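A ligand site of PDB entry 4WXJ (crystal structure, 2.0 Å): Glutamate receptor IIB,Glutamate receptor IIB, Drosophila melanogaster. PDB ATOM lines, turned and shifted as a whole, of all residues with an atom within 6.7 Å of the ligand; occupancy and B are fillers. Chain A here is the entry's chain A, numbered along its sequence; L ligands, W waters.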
ATOM      1  N   TYR A  68      24.863  -9.748 -20.869  1.00  0.00           N
ATOM      2  CA  TYR A  68      25.953 -10.439 -21.551  1.00  0.00           C
ATOM      3  C   TYR A  68      25.496 -10.903 -22.924  1.00  0.00           C
ATOM      4  O   TYR A  68      26.069 -10.517 -23.946  1.00  0.00           O
ATOM      5  CB  TYR A  68      26.437 -11.646 -20.743  1.00  0.00           C
ATOM      6  CG  TYR A  68      27.162 -11.315 -19.454  1.00  0.00           C
ATOM      7  CD1 TYR A  68      26.467 -11.101 -18.274  1.00  0.00           C
ATOM      8  CD2 TYR A  68      28.544 -11.250 -19.424  1.00  0.00           C
ATOM      9  CE1 TYR A  68      27.131 -10.814 -17.096  1.00  0.00           C
ATOM     10  CE2 TYR A  68      29.228 -10.969 -18.254  1.00  0.00           C
ATOM     11  CZ  TYR A  68      28.514 -10.751 -17.088  1.00  0.00           C
ATOM     12  OH  TYR A  68      29.176 -10.461 -15.920  1.00  0.00           O
ATOM     13  N   GLY A  69      24.450 -11.732 -22.936  1.00  0.00           N
ATOM     14  CA  GLY A  69      23.922 -12.289 -24.163  1.00  0.00           C
ATOM     15  C   GLY A  69      23.492 -13.733 -23.983  1.00  0.00           C
ATOM     16  O   GLY A  69      24.322 -14.609 -23.743  1.00  0.00           O
ATOM     17  N   CYS A  95      33.984  -7.989 -22.497  1.00  0.00           N
ATOM     18  CA  CYS A  95      33.842  -7.859 -21.041  1.00  0.00           C
ATOM     19  C   CYS A  95      34.318  -9.205 -20.489  1.00  0.00           C
ATOM     20  O   CYS A  95      35.119  -9.874 -21.128  1.00  0.00           O
ATOM     21  CB  CYS A  95      32.405  -7.559 -20.604  1.00  0.00           C
ATOM     22  SG  CYS A  95      31.199  -8.815 -21.060  1.00  0.00           S
ATOM     23  N   ASP A  96      33.812  -9.612 -19.330  1.00  0.00           N
ATOM     24  CA  ASP A  96      33.966 -10.998 -18.902  1.00  0.00           C
ATOM     25  C   ASP A  96      33.007 -11.849 -19.732  1.00  0.00           C
ATOM     26  O   ASP A  96      32.047 -12.403 -19.220  1.00  0.00           O
ATOM     27  CB  ASP A  96      33.689 -11.178 -17.410  1.00  0.00           C
ATOM     28  CG  ASP A  96      32.401 -10.522 -16.960  1.00  0.00           C
ATOM     29  OD1 ASP A  96      32.044  -9.454 -17.517  1.00  0.00           O
ATOM     30  OD2 ASP A  96      31.750 -11.065 -16.051  1.00  0.00           O
ATOM     31  N   LEU A  97      33.298 -11.939 -21.027  1.00  0.00           N
ATOM     32  CA  LEU A  97      32.421 -12.603 -21.972  1.00  0.00           C
ATOM     33  C   LEU A  97      32.910 -14.021 -22.208  1.00  0.00           C
ATOM     34  O   LEU A  97      33.890 -14.253 -22.918  1.00  0.00           O
ATOM     35  CB  LEU A  97      32.368 -11.819 -23.289  1.00  0.00           C
ATOM     36  CG  LEU A  97      31.285 -12.218 -24.304  1.00  0.00           C
ATOM     37  CD1 LEU A  97      29.888 -12.014 -23.742  1.00  0.00           C
ATOM     38  CD2 LEU A  97      31.469 -11.423 -25.588  1.00  0.00           C
ATOM     39  N   THR A  98      32.228 -14.976 -21.594  1.00  0.00           N
ATOM     40  CA  THR A  98      32.638 -16.371 -21.643  1.00  0.00           C
ATOM     41  C   THR A  98      32.232 -17.035 -22.952  1.00  0.00           C
ATOM     42  O   THR A  98      31.116 -16.838 -23.438  1.00  0.00           O
ATOM     43  CB  THR A  98      32.019 -17.157 -20.472  1.00  0.00           C
ATOM     44  OG1 THR A  98      32.360 -16.515 -19.236  1.00  0.00           O
ATOM     45  CG2 THR A  98      32.541 -18.597 -20.457  1.00  0.00           C
ATOM     46  N   ILE A  99      33.144 -17.821 -23.501  1.00  0.00           N
ATOM     47  CA  ILE A  99      32.869 -18.549 -24.733  1.00  0.00           C
ATOM     48  C   ILE A  99      31.979 -19.754 -24.453  1.00  0.00           C
ATOM     49  O   ILE A  99      32.346 -20.644 -23.686  1.00  0.00           O
ATOM     50  CB  ILE A  99      34.177 -19.018 -25.410  1.00  0.00           C
ATOM     51  CG1 ILE A  99      35.054 -17.801 -25.737  1.00  0.00           C
ATOM     52  CG2 ILE A  99      33.874 -19.807 -26.682  1.00  0.00           C
ATOM     53  CD1 ILE A  99      36.445 -18.145 -26.256  1.00  0.00           C
ATOM     54  N   THR A 100      30.798 -19.760 -25.079  1.00  0.00           N
ATOM     55  CA  THR A 100      29.872 -20.876 -24.959  1.00  0.00           C
ATOM     56  C   THR A 100      29.488 -21.389 -26.333  1.00  0.00           C
ATOM     57  O   THR A 100      29.639 -20.691 -27.333  1.00  0.00           O
ATOM     58  CB  THR A 100      28.579 -20.478 -24.198  1.00  0.00           C
ATOM     59  OG1 THR A 100      27.819 -19.576 -25.004  1.00  0.00           O
ATOM     60  CG2 THR A 100      28.917 -19.812 -22.870  1.00  0.00           C
ATOM     61  N   ARG A 103      26.736 -19.303 -28.060  1.00  0.00           N
ATOM     62  CA  ARG A 103      27.239 -18.012 -28.521  1.00  0.00           C
ATOM     63  C   ARG A 103      28.110 -18.168 -29.758  1.00  0.00           C
ATOM     64  O   ARG A 103      28.005 -17.395 -30.712  1.00  0.00           O
ATOM     65  CB  ARG A 103      28.016 -17.318 -27.414  1.00  0.00           C
ATOM     66  CG  ARG A 103      27.146 -16.812 -26.273  1.00  0.00           C
ATOM     67  CD  ARG A 103      27.977 -16.323 -25.114  1.00  0.00           C
ATOM     68  NE  ARG A 103      27.145 -15.759 -24.054  1.00  0.00           N
ATOM     69  CZ  ARG A 103      27.617 -15.395 -22.859  1.00  0.00           C
ATOM     70  NH1 ARG A 103      28.892 -15.554 -22.566  1.00  0.00           N
ATOM     71  NH2 ARG A 103      26.785 -14.884 -21.951  1.00  0.00           N
ATOM     72  N   LEU A 116      39.831 -19.221 -16.869  1.00  0.00           N
ATOM     73  CA  LEU A 116      39.198 -19.158 -15.561  1.00  0.00           C
ATOM     74  C   LEU A 116      38.453 -20.459 -15.259  1.00  0.00           C
ATOM     75  O   LEU A 116      38.466 -21.403 -16.048  1.00  0.00           O
ATOM     76  CB  LEU A 116      38.228 -17.981 -15.507  1.00  0.00           C
ATOM     77  CG  LEU A 116      37.223 -17.925 -16.666  1.00  0.00           C
ATOM     78  CD1 LEU A 116      35.841 -17.534 -16.169  1.00  0.00           C
ATOM     79  CD2 LEU A 116      37.702 -16.967 -17.746  1.00  0.00           C
ATOM     80  N   ILE A 118      35.000 -22.018 -12.380  1.00  0.00           N
ATOM     81  CA  ILE A 118      33.802 -21.709 -11.613  1.00  0.00           C
ATOM     82  C   ILE A 118      34.014 -22.142 -10.168  1.00  0.00           C
ATOM     83  O   ILE A 118      34.695 -23.120  -9.902  1.00  0.00           O
ATOM     84  CB  ILE A 118      32.564 -22.418 -12.192  1.00  0.00           C
ATOM     85  CG1 ILE A 118      32.288 -21.945 -13.631  1.00  0.00           C
ATOM     86  CG2 ILE A 118      31.333 -22.186 -11.328  1.00  0.00           C
ATOM     87  CD1 ILE A 118      31.287 -22.803 -14.376  1.00  0.00           C
ATOM     88  N   THR A 144      22.824 -18.839  -9.876  1.00  0.00           N
ATOM     89  CA  THR A 144      23.766 -18.213 -10.802  1.00  0.00           C
ATOM     90  C   THR A 144      23.130 -17.010 -11.472  1.00  0.00           C
ATOM     91  O   THR A 144      21.979 -16.676 -11.224  1.00  0.00           O
ATOM     92  CB  THR A 144      24.220 -19.196 -11.902  1.00  0.00           C
ATOM     93  OG1 THR A 144      23.109 -19.512 -12.761  1.00  0.00           O
ATOM     94  CG2 THR A 144      24.769 -20.485 -11.303  1.00  0.00           C
ATOM     95  N   ILE A 145      23.897 -16.354 -12.343  1.00  0.00           N
ATOM     96  CA  ILE A 145      23.350 -15.302 -13.182  1.00  0.00           C
ATOM     97  C   ILE A 145      22.413 -15.920 -14.216  1.00  0.00           C
ATOM     98  O   ILE A 145      22.745 -16.908 -14.858  1.00  0.00           O
ATOM     99  CB  ILE A 145      24.446 -14.506 -13.885  1.00  0.00           C
ATOM    100  CG1 ILE A 145      25.255 -13.719 -12.849  1.00  0.00           C
ATOM    101  CG2 ILE A 145      23.856 -13.551 -14.927  1.00  0.00           C
ATOM    102  CD1 ILE A 145      26.554 -13.150 -13.386  1.00  0.00           C
ATOM    103  N   GLY A 147      20.743 -16.906 -17.376  1.00  0.00           N
ATOM    104  CA  GLY A 147      21.169 -16.972 -18.767  1.00  0.00           C
ATOM    105  C   GLY A 147      22.653 -16.749 -18.960  1.00  0.00           C
ATOM    106  O   GLY A 147      23.109 -16.582 -20.099  1.00  0.00           O
ATOM    107  N   GLY A 148      23.418 -16.738 -17.878  1.00  0.00           N
ATOM    108  CA  GLY A 148      24.855 -16.546 -17.949  1.00  0.00           C
ATOM    109  C   GLY A 148      25.582 -17.831 -18.314  1.00  0.00           C
ATOM    110  O   GLY A 148      24.953 -18.883 -18.452  1.00  0.00           O
ATOM    111  N   ALA A 149      26.896 -17.745 -18.452  1.00  0.00           N
ATOM    112  CA  ALA A 149      27.693 -18.900 -18.868  1.00  0.00           C
ATOM    113  C   ALA A 149      27.808 -19.941 -17.759  1.00  0.00           C
ATOM    114  O   ALA A 149      27.989 -21.129 -18.036  1.00  0.00           O
ATOM    115  CB  ALA A 149      29.068 -18.453 -19.308  1.00  0.00           C
ATOM    116  N   THR A 150      27.725 -19.517 -16.503  1.00  0.00           N
ATOM    117  CA  THR A 150      27.806 -20.461 -15.392  1.00  0.00           C
ATOM    118  C   THR A 150      26.546 -21.322 -15.353  1.00  0.00           C
ATOM    119  O   THR A 150      26.596 -22.493 -14.971  1.00  0.00           O
ATOM    120  CB  THR A 150      28.010 -19.739 -14.046  1.00  0.00           C
ATOM    121  OG1 THR A 150      29.247 -19.015 -14.081  1.00  0.00           O
ATOM    122  CG2 THR A 150      28.053 -20.744 -12.908  1.00  0.00           C
ATOM    123  N   SER A 151      25.406 -20.738 -15.739  1.00  0.00           N
ATOM    124  CA  SER A 151      24.180 -21.513 -15.900  1.00  0.00           C
ATOM    125  C   SER A 151      24.374 -22.594 -16.954  1.00  0.00           C
ATOM    126  O   SER A 151      23.870 -23.710 -16.822  1.00  0.00           O
ATOM    127  CB  SER A 151      23.018 -20.610 -16.308  1.00  0.00           C
ATOM    128  OG  SER A 151      22.506 -19.904 -15.185  1.00  0.00           O
ATOM    129  N   ASN A 181      26.518 -10.184 -11.489  1.00  0.00           N
ATOM    130  CA  ASN A 181      27.425 -10.504 -10.377  1.00  0.00           C
ATOM    131  C   ASN A 181      27.131  -9.659  -9.141  1.00  0.00           C
ATOM    132  O   ASN A 181      27.200 -10.147  -8.022  1.00  0.00           O
ATOM    133  CB  ASN A 181      28.881 -10.307 -10.804  1.00  0.00           C
ATOM    134  CG  ASN A 181      29.375 -11.397 -11.729  1.00  0.00           C
ATOM    135  OD1 ASN A 181      29.893 -11.132 -12.808  1.00  0.00           O
ATOM    136  ND2 ASN A 181      29.232 -12.653 -11.293  1.00  0.00           N
ATOM    137  N   PHE A 197      26.515 -18.246  -3.946  1.00  0.00           N
ATOM    138  CA  PHE A 197      26.497 -17.783  -5.330  1.00  0.00           C
ATOM    139  C   PHE A 197      27.545 -18.510  -6.159  1.00  0.00           C
ATOM    140  O   PHE A 197      28.735 -18.444  -5.872  1.00  0.00           O
ATOM    141  CB  PHE A 197      26.717 -16.266  -5.371  1.00  0.00           C
ATOM    142  CG  PHE A 197      26.480 -15.653  -6.733  1.00  0.00           C
ATOM    143  CD1 PHE A 197      25.280 -15.861  -7.391  1.00  0.00           C
ATOM    144  CD2 PHE A 197      27.432 -14.842  -7.318  1.00  0.00           C
ATOM    145  CE1 PHE A 197      25.051 -15.295  -8.639  1.00  0.00           C
ATOM    146  CE2 PHE A 197      27.214 -14.272  -8.557  1.00  0.00           C
ATOM    147  CZ  PHE A 197      26.028 -14.497  -9.213  1.00  0.00           C
ATOM    148  N   LEU A 198      27.085 -19.218  -7.186  1.00  0.00           N
ATOM    149  CA  LEU A 198      27.964 -19.913  -8.098  1.00  0.00           C
ATOM    150  C   LEU A 198      28.391 -18.945  -9.204  1.00  0.00           C
ATOM    151  O   LEU A 198      27.559 -18.404  -9.930  1.00  0.00           O
ATOM    152  CB  LEU A 198      27.271 -21.143  -8.689  1.00  0.00           C
ATOM    153  CG  LEU A 198      27.127 -22.310  -7.709  1.00  0.00           C
ATOM    154  CD1 LEU A 198      25.787 -22.991  -7.892  1.00  0.00           C
ATOM    155  CD2 LEU A 198      28.267 -23.292  -7.880  1.00  0.00           C
ATOM    156  N   MET A 199      29.699 -18.733  -9.320  1.00  0.00           N
ATOM    157  CA  MET A 199      30.233 -17.705 -10.206  1.00  0.00           C
ATOM    158  C   MET A 199      31.626 -18.049 -10.694  1.00  0.00           C
ATOM    159  O   MET A 199      32.236 -19.014 -10.235  1.00  0.00           O
ATOM    160  CB  MET A 199      30.249 -16.354  -9.496  1.00  0.00           C
ATOM    161  CG  MET A 199      31.181 -16.311  -8.292  1.00  0.00           C
ATOM    162  SD  MET A 199      30.943 -14.844  -7.260  1.00  0.00           S
ATOM    163  CE  MET A 199      31.253 -13.530  -8.441  1.00  0.00           C
ATOM    164  N   GLU A 200      32.121 -17.248 -11.625  1.00  0.00           N
ATOM    165  CA  GLU A 200      33.423 -17.469 -12.207  1.00  0.00           C
ATOM    166  C   GLU A 200      34.525 -16.990 -11.263  1.00  0.00           C
ATOM    167  O   GLU A 200      34.364 -15.993 -10.559  1.00  0.00           O
ATOM    168  CB  GLU A 200      33.513 -16.767 -13.562  1.00  0.00           C
ATOM    169  CG  GLU A 200      32.596 -17.408 -14.597  1.00  0.00           C
ATOM    170  CD  GLU A 200      32.460 -16.590 -15.872  1.00  0.00           C
ATOM    171  OE1 GLU A 200      32.752 -15.383 -15.849  1.00  0.00           O
ATOM    172  OE2 GLU A 200      32.045 -17.170 -16.902  1.00  0.00           O
ATOM    173  N   ASN A 203      35.719 -13.228 -11.192  1.00  0.00           N
ATOM    174  CA  ASN A 203      34.808 -12.304 -10.513  1.00  0.00           C
ATOM    175  C   ASN A 203      34.726 -12.592  -9.027  1.00  0.00           C
ATOM    176  O   ASN A 203      34.585 -11.671  -8.219  1.00  0.00           O
ATOM    177  CB  ASN A 203      33.419 -12.394 -11.145  1.00  0.00           C
ATOM    178  CG  ASN A 203      33.425 -12.051 -12.618  1.00  0.00           C
ATOM    179  OD1 ASN A 203      34.183 -11.184 -13.061  1.00  0.00           O
ATOM    180  ND2 ASN A 203      32.580 -12.727 -13.393  1.00  0.00           N
ATOM    181  N   TYR A 226      37.545 -16.300 -21.429  1.00  0.00           N
ATOM    182  CA  TYR A 226      37.018 -15.030 -21.922  1.00  0.00           C
ATOM    183  C   TYR A 226      37.617 -14.735 -23.293  1.00  0.00           C
ATOM    184  O   TYR A 226      38.832 -14.854 -23.485  1.00  0.00           O
ATOM    185  CB  TYR A 226      37.351 -13.877 -20.985  1.00  0.00           C
ATOM    186  CG  TYR A 226      36.704 -13.927 -19.615  1.00  0.00           C
ATOM    187  CD1 TYR A 226      35.540 -14.660 -19.400  1.00  0.00           C
ATOM    188  CD2 TYR A 226      37.248 -13.234 -18.551  1.00  0.00           C
ATOM    189  CE1 TYR A 226      34.951 -14.705 -18.141  1.00  0.00           C
ATOM    190  CE2 TYR A 226      36.664 -13.270 -17.302  1.00  0.00           C
ATOM    191  CZ  TYR A 226      35.517 -14.008 -17.103  1.00  0.00           C
ATOM    192  OH  TYR A 226      34.947 -14.030 -15.855  1.00  0.00           O
HETATM  193  N1  LIG L   1      31.062 -14.488 -17.989  1.00  0.00           N
HETATM  194  C1  LIG L   1      29.691 -15.048 -17.920  1.00  0.00           C
HETATM  195  C2  LIG L   1      29.016 -14.965 -19.291  1.00  0.00           C
HETATM  196  O1  LIG L   1      29.657 -14.621 -20.278  1.00  0.00           O
HETATM  197  C3  LIG L   1      28.867 -14.317 -16.865  1.00  0.00           C
HETATM  198  C4  LIG L   1      29.248 -14.638 -15.428  1.00  0.00           C
HETATM  199  C5  LIG L   1      28.647 -15.939 -14.921  1.00  0.00           C
HETATM  200  O2  LIG L   1      29.050 -16.377 -13.818  1.00  0.00           O
HETATM  201  O3  LIG L   1      27.778 -16.524 -15.604  1.00  0.00           O
HETATM  202  O4  LIG L   1      27.819 -15.237 -19.434  1.00  0.00           O
HETATM  203  O   HOH W   1      26.831 -16.693 -12.358  1.00  0.00           O
HETATM  204  O   HOH W   2      25.351 -17.823 -15.170  1.00  0.00           O
HETATM  205  O   HOH W   3      30.651 -14.682 -12.607  1.00  0.00           O
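The side-chain carboxylate (OE1) of Glu 200 lies within salt-bridge range of a nitrogen (N1) of the ligand.
A nitrogen (N1) of the ligand lies within hydrogen-bond range of the backbone carbonyl oxygen (O) of Asp 96 (2.6 Å).
NH1 of Arg 103 lies within salt-bridge range of O1 of the ligand.
OD2 of Asp 96 lies within salt-bridge range of N1 of the ligand (3.99 Å).
The backbone NH (N) of Thr 150 lies within hydrogen-bond range of an oxygen (O3) of the ligand (3.1 Å).
N of Thr 98 lies within hydrogen-bond range of O1 of the ligand (2.9 Å).
N of Ala 149 lies within hydrogen-bond range of O4 of the ligand.
N1 of the ligand lies within hydrogen-bond range of OG1 of Thr 98 (2.7 Å).
The side-chain hydroxyl of Thr 150 sits at hydrogen-bond distance from an oxygen (O2) of the ligand (2.7 Å).
SG of Cys 95 sits close to N of Leu 97, 3.8 Å away.
The backbone carbonyl oxygen of Gly 69 lies within hydrogen-bond range of the guanidinium group of Arg 103.
The side-chain sulfur (SG) of Cys 95 lies close to the side-chain carboxylate (OD1) of Asp 96 (3.7 Å).
O of Ile 145 sits at hydrogen-bond distance from OG of Ser 151, 3.0 Å away.
The side-chain carboxylate (OE2) of Glu 200 sits at hydrogen-bond distance from the side-chain hydroxyl (OG1) of Thr 98.
OH of Tyr 68 sits at hydrogen-bond distance from OD2 of Asp 96, 2.6 Å away.
The side-chain carboxylate of Glu 200 is in hydrogen-bond range of the side-chain hydroxyl of Tyr 226 (2.6 Å).
OH of Tyr 68 sits at hydrogen-bond distance from OD1 of Asn 181 (3.3 Å).
Tyr 68 touches the ligand (CZ to C3, 3.6 Å).
CA of Leu 97 touches O1 of the ligand, 3.8 Å away.
Ile 145 touches the ligand.
Gly 148 touches the ligand (CA to O4, 3.6 Å).
CE1 of Tyr 226 touches N1 of the ligand, 3.9 Å away.
Hydrophobic or aromatic side chains within 4 Å of the ligand: Tyr 68, Ile 145, Ala 149 and Tyr 226.
11 residues have an atom within 4 Å of the ligand: Tyr 68, Asp 96, Leu 97, Thr 98, Arg 103, Ile 145, Gly 148, Ala 149, Thr 150, Glu 200 and Tyr 226.
Water W1 lies within hydrogen-bond range of an oxygen (O2) of the ligand, the backbone NH (N) of Ile 145 and the backbone carbonyl oxygen (O) of Leu 198.
Water W2 lies within hydrogen-bond range of the backbone carbonyl oxygen of Ile 145 (2.8 Å), an oxygen (O3) of the ligand (2.8 Å), the backbone NH of Ser 151 (3.0 Å), the backbone NH of Thr 150 (3.2 Å) and the backbone carbonyl oxygen of Gly 148 (3.5 Å).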
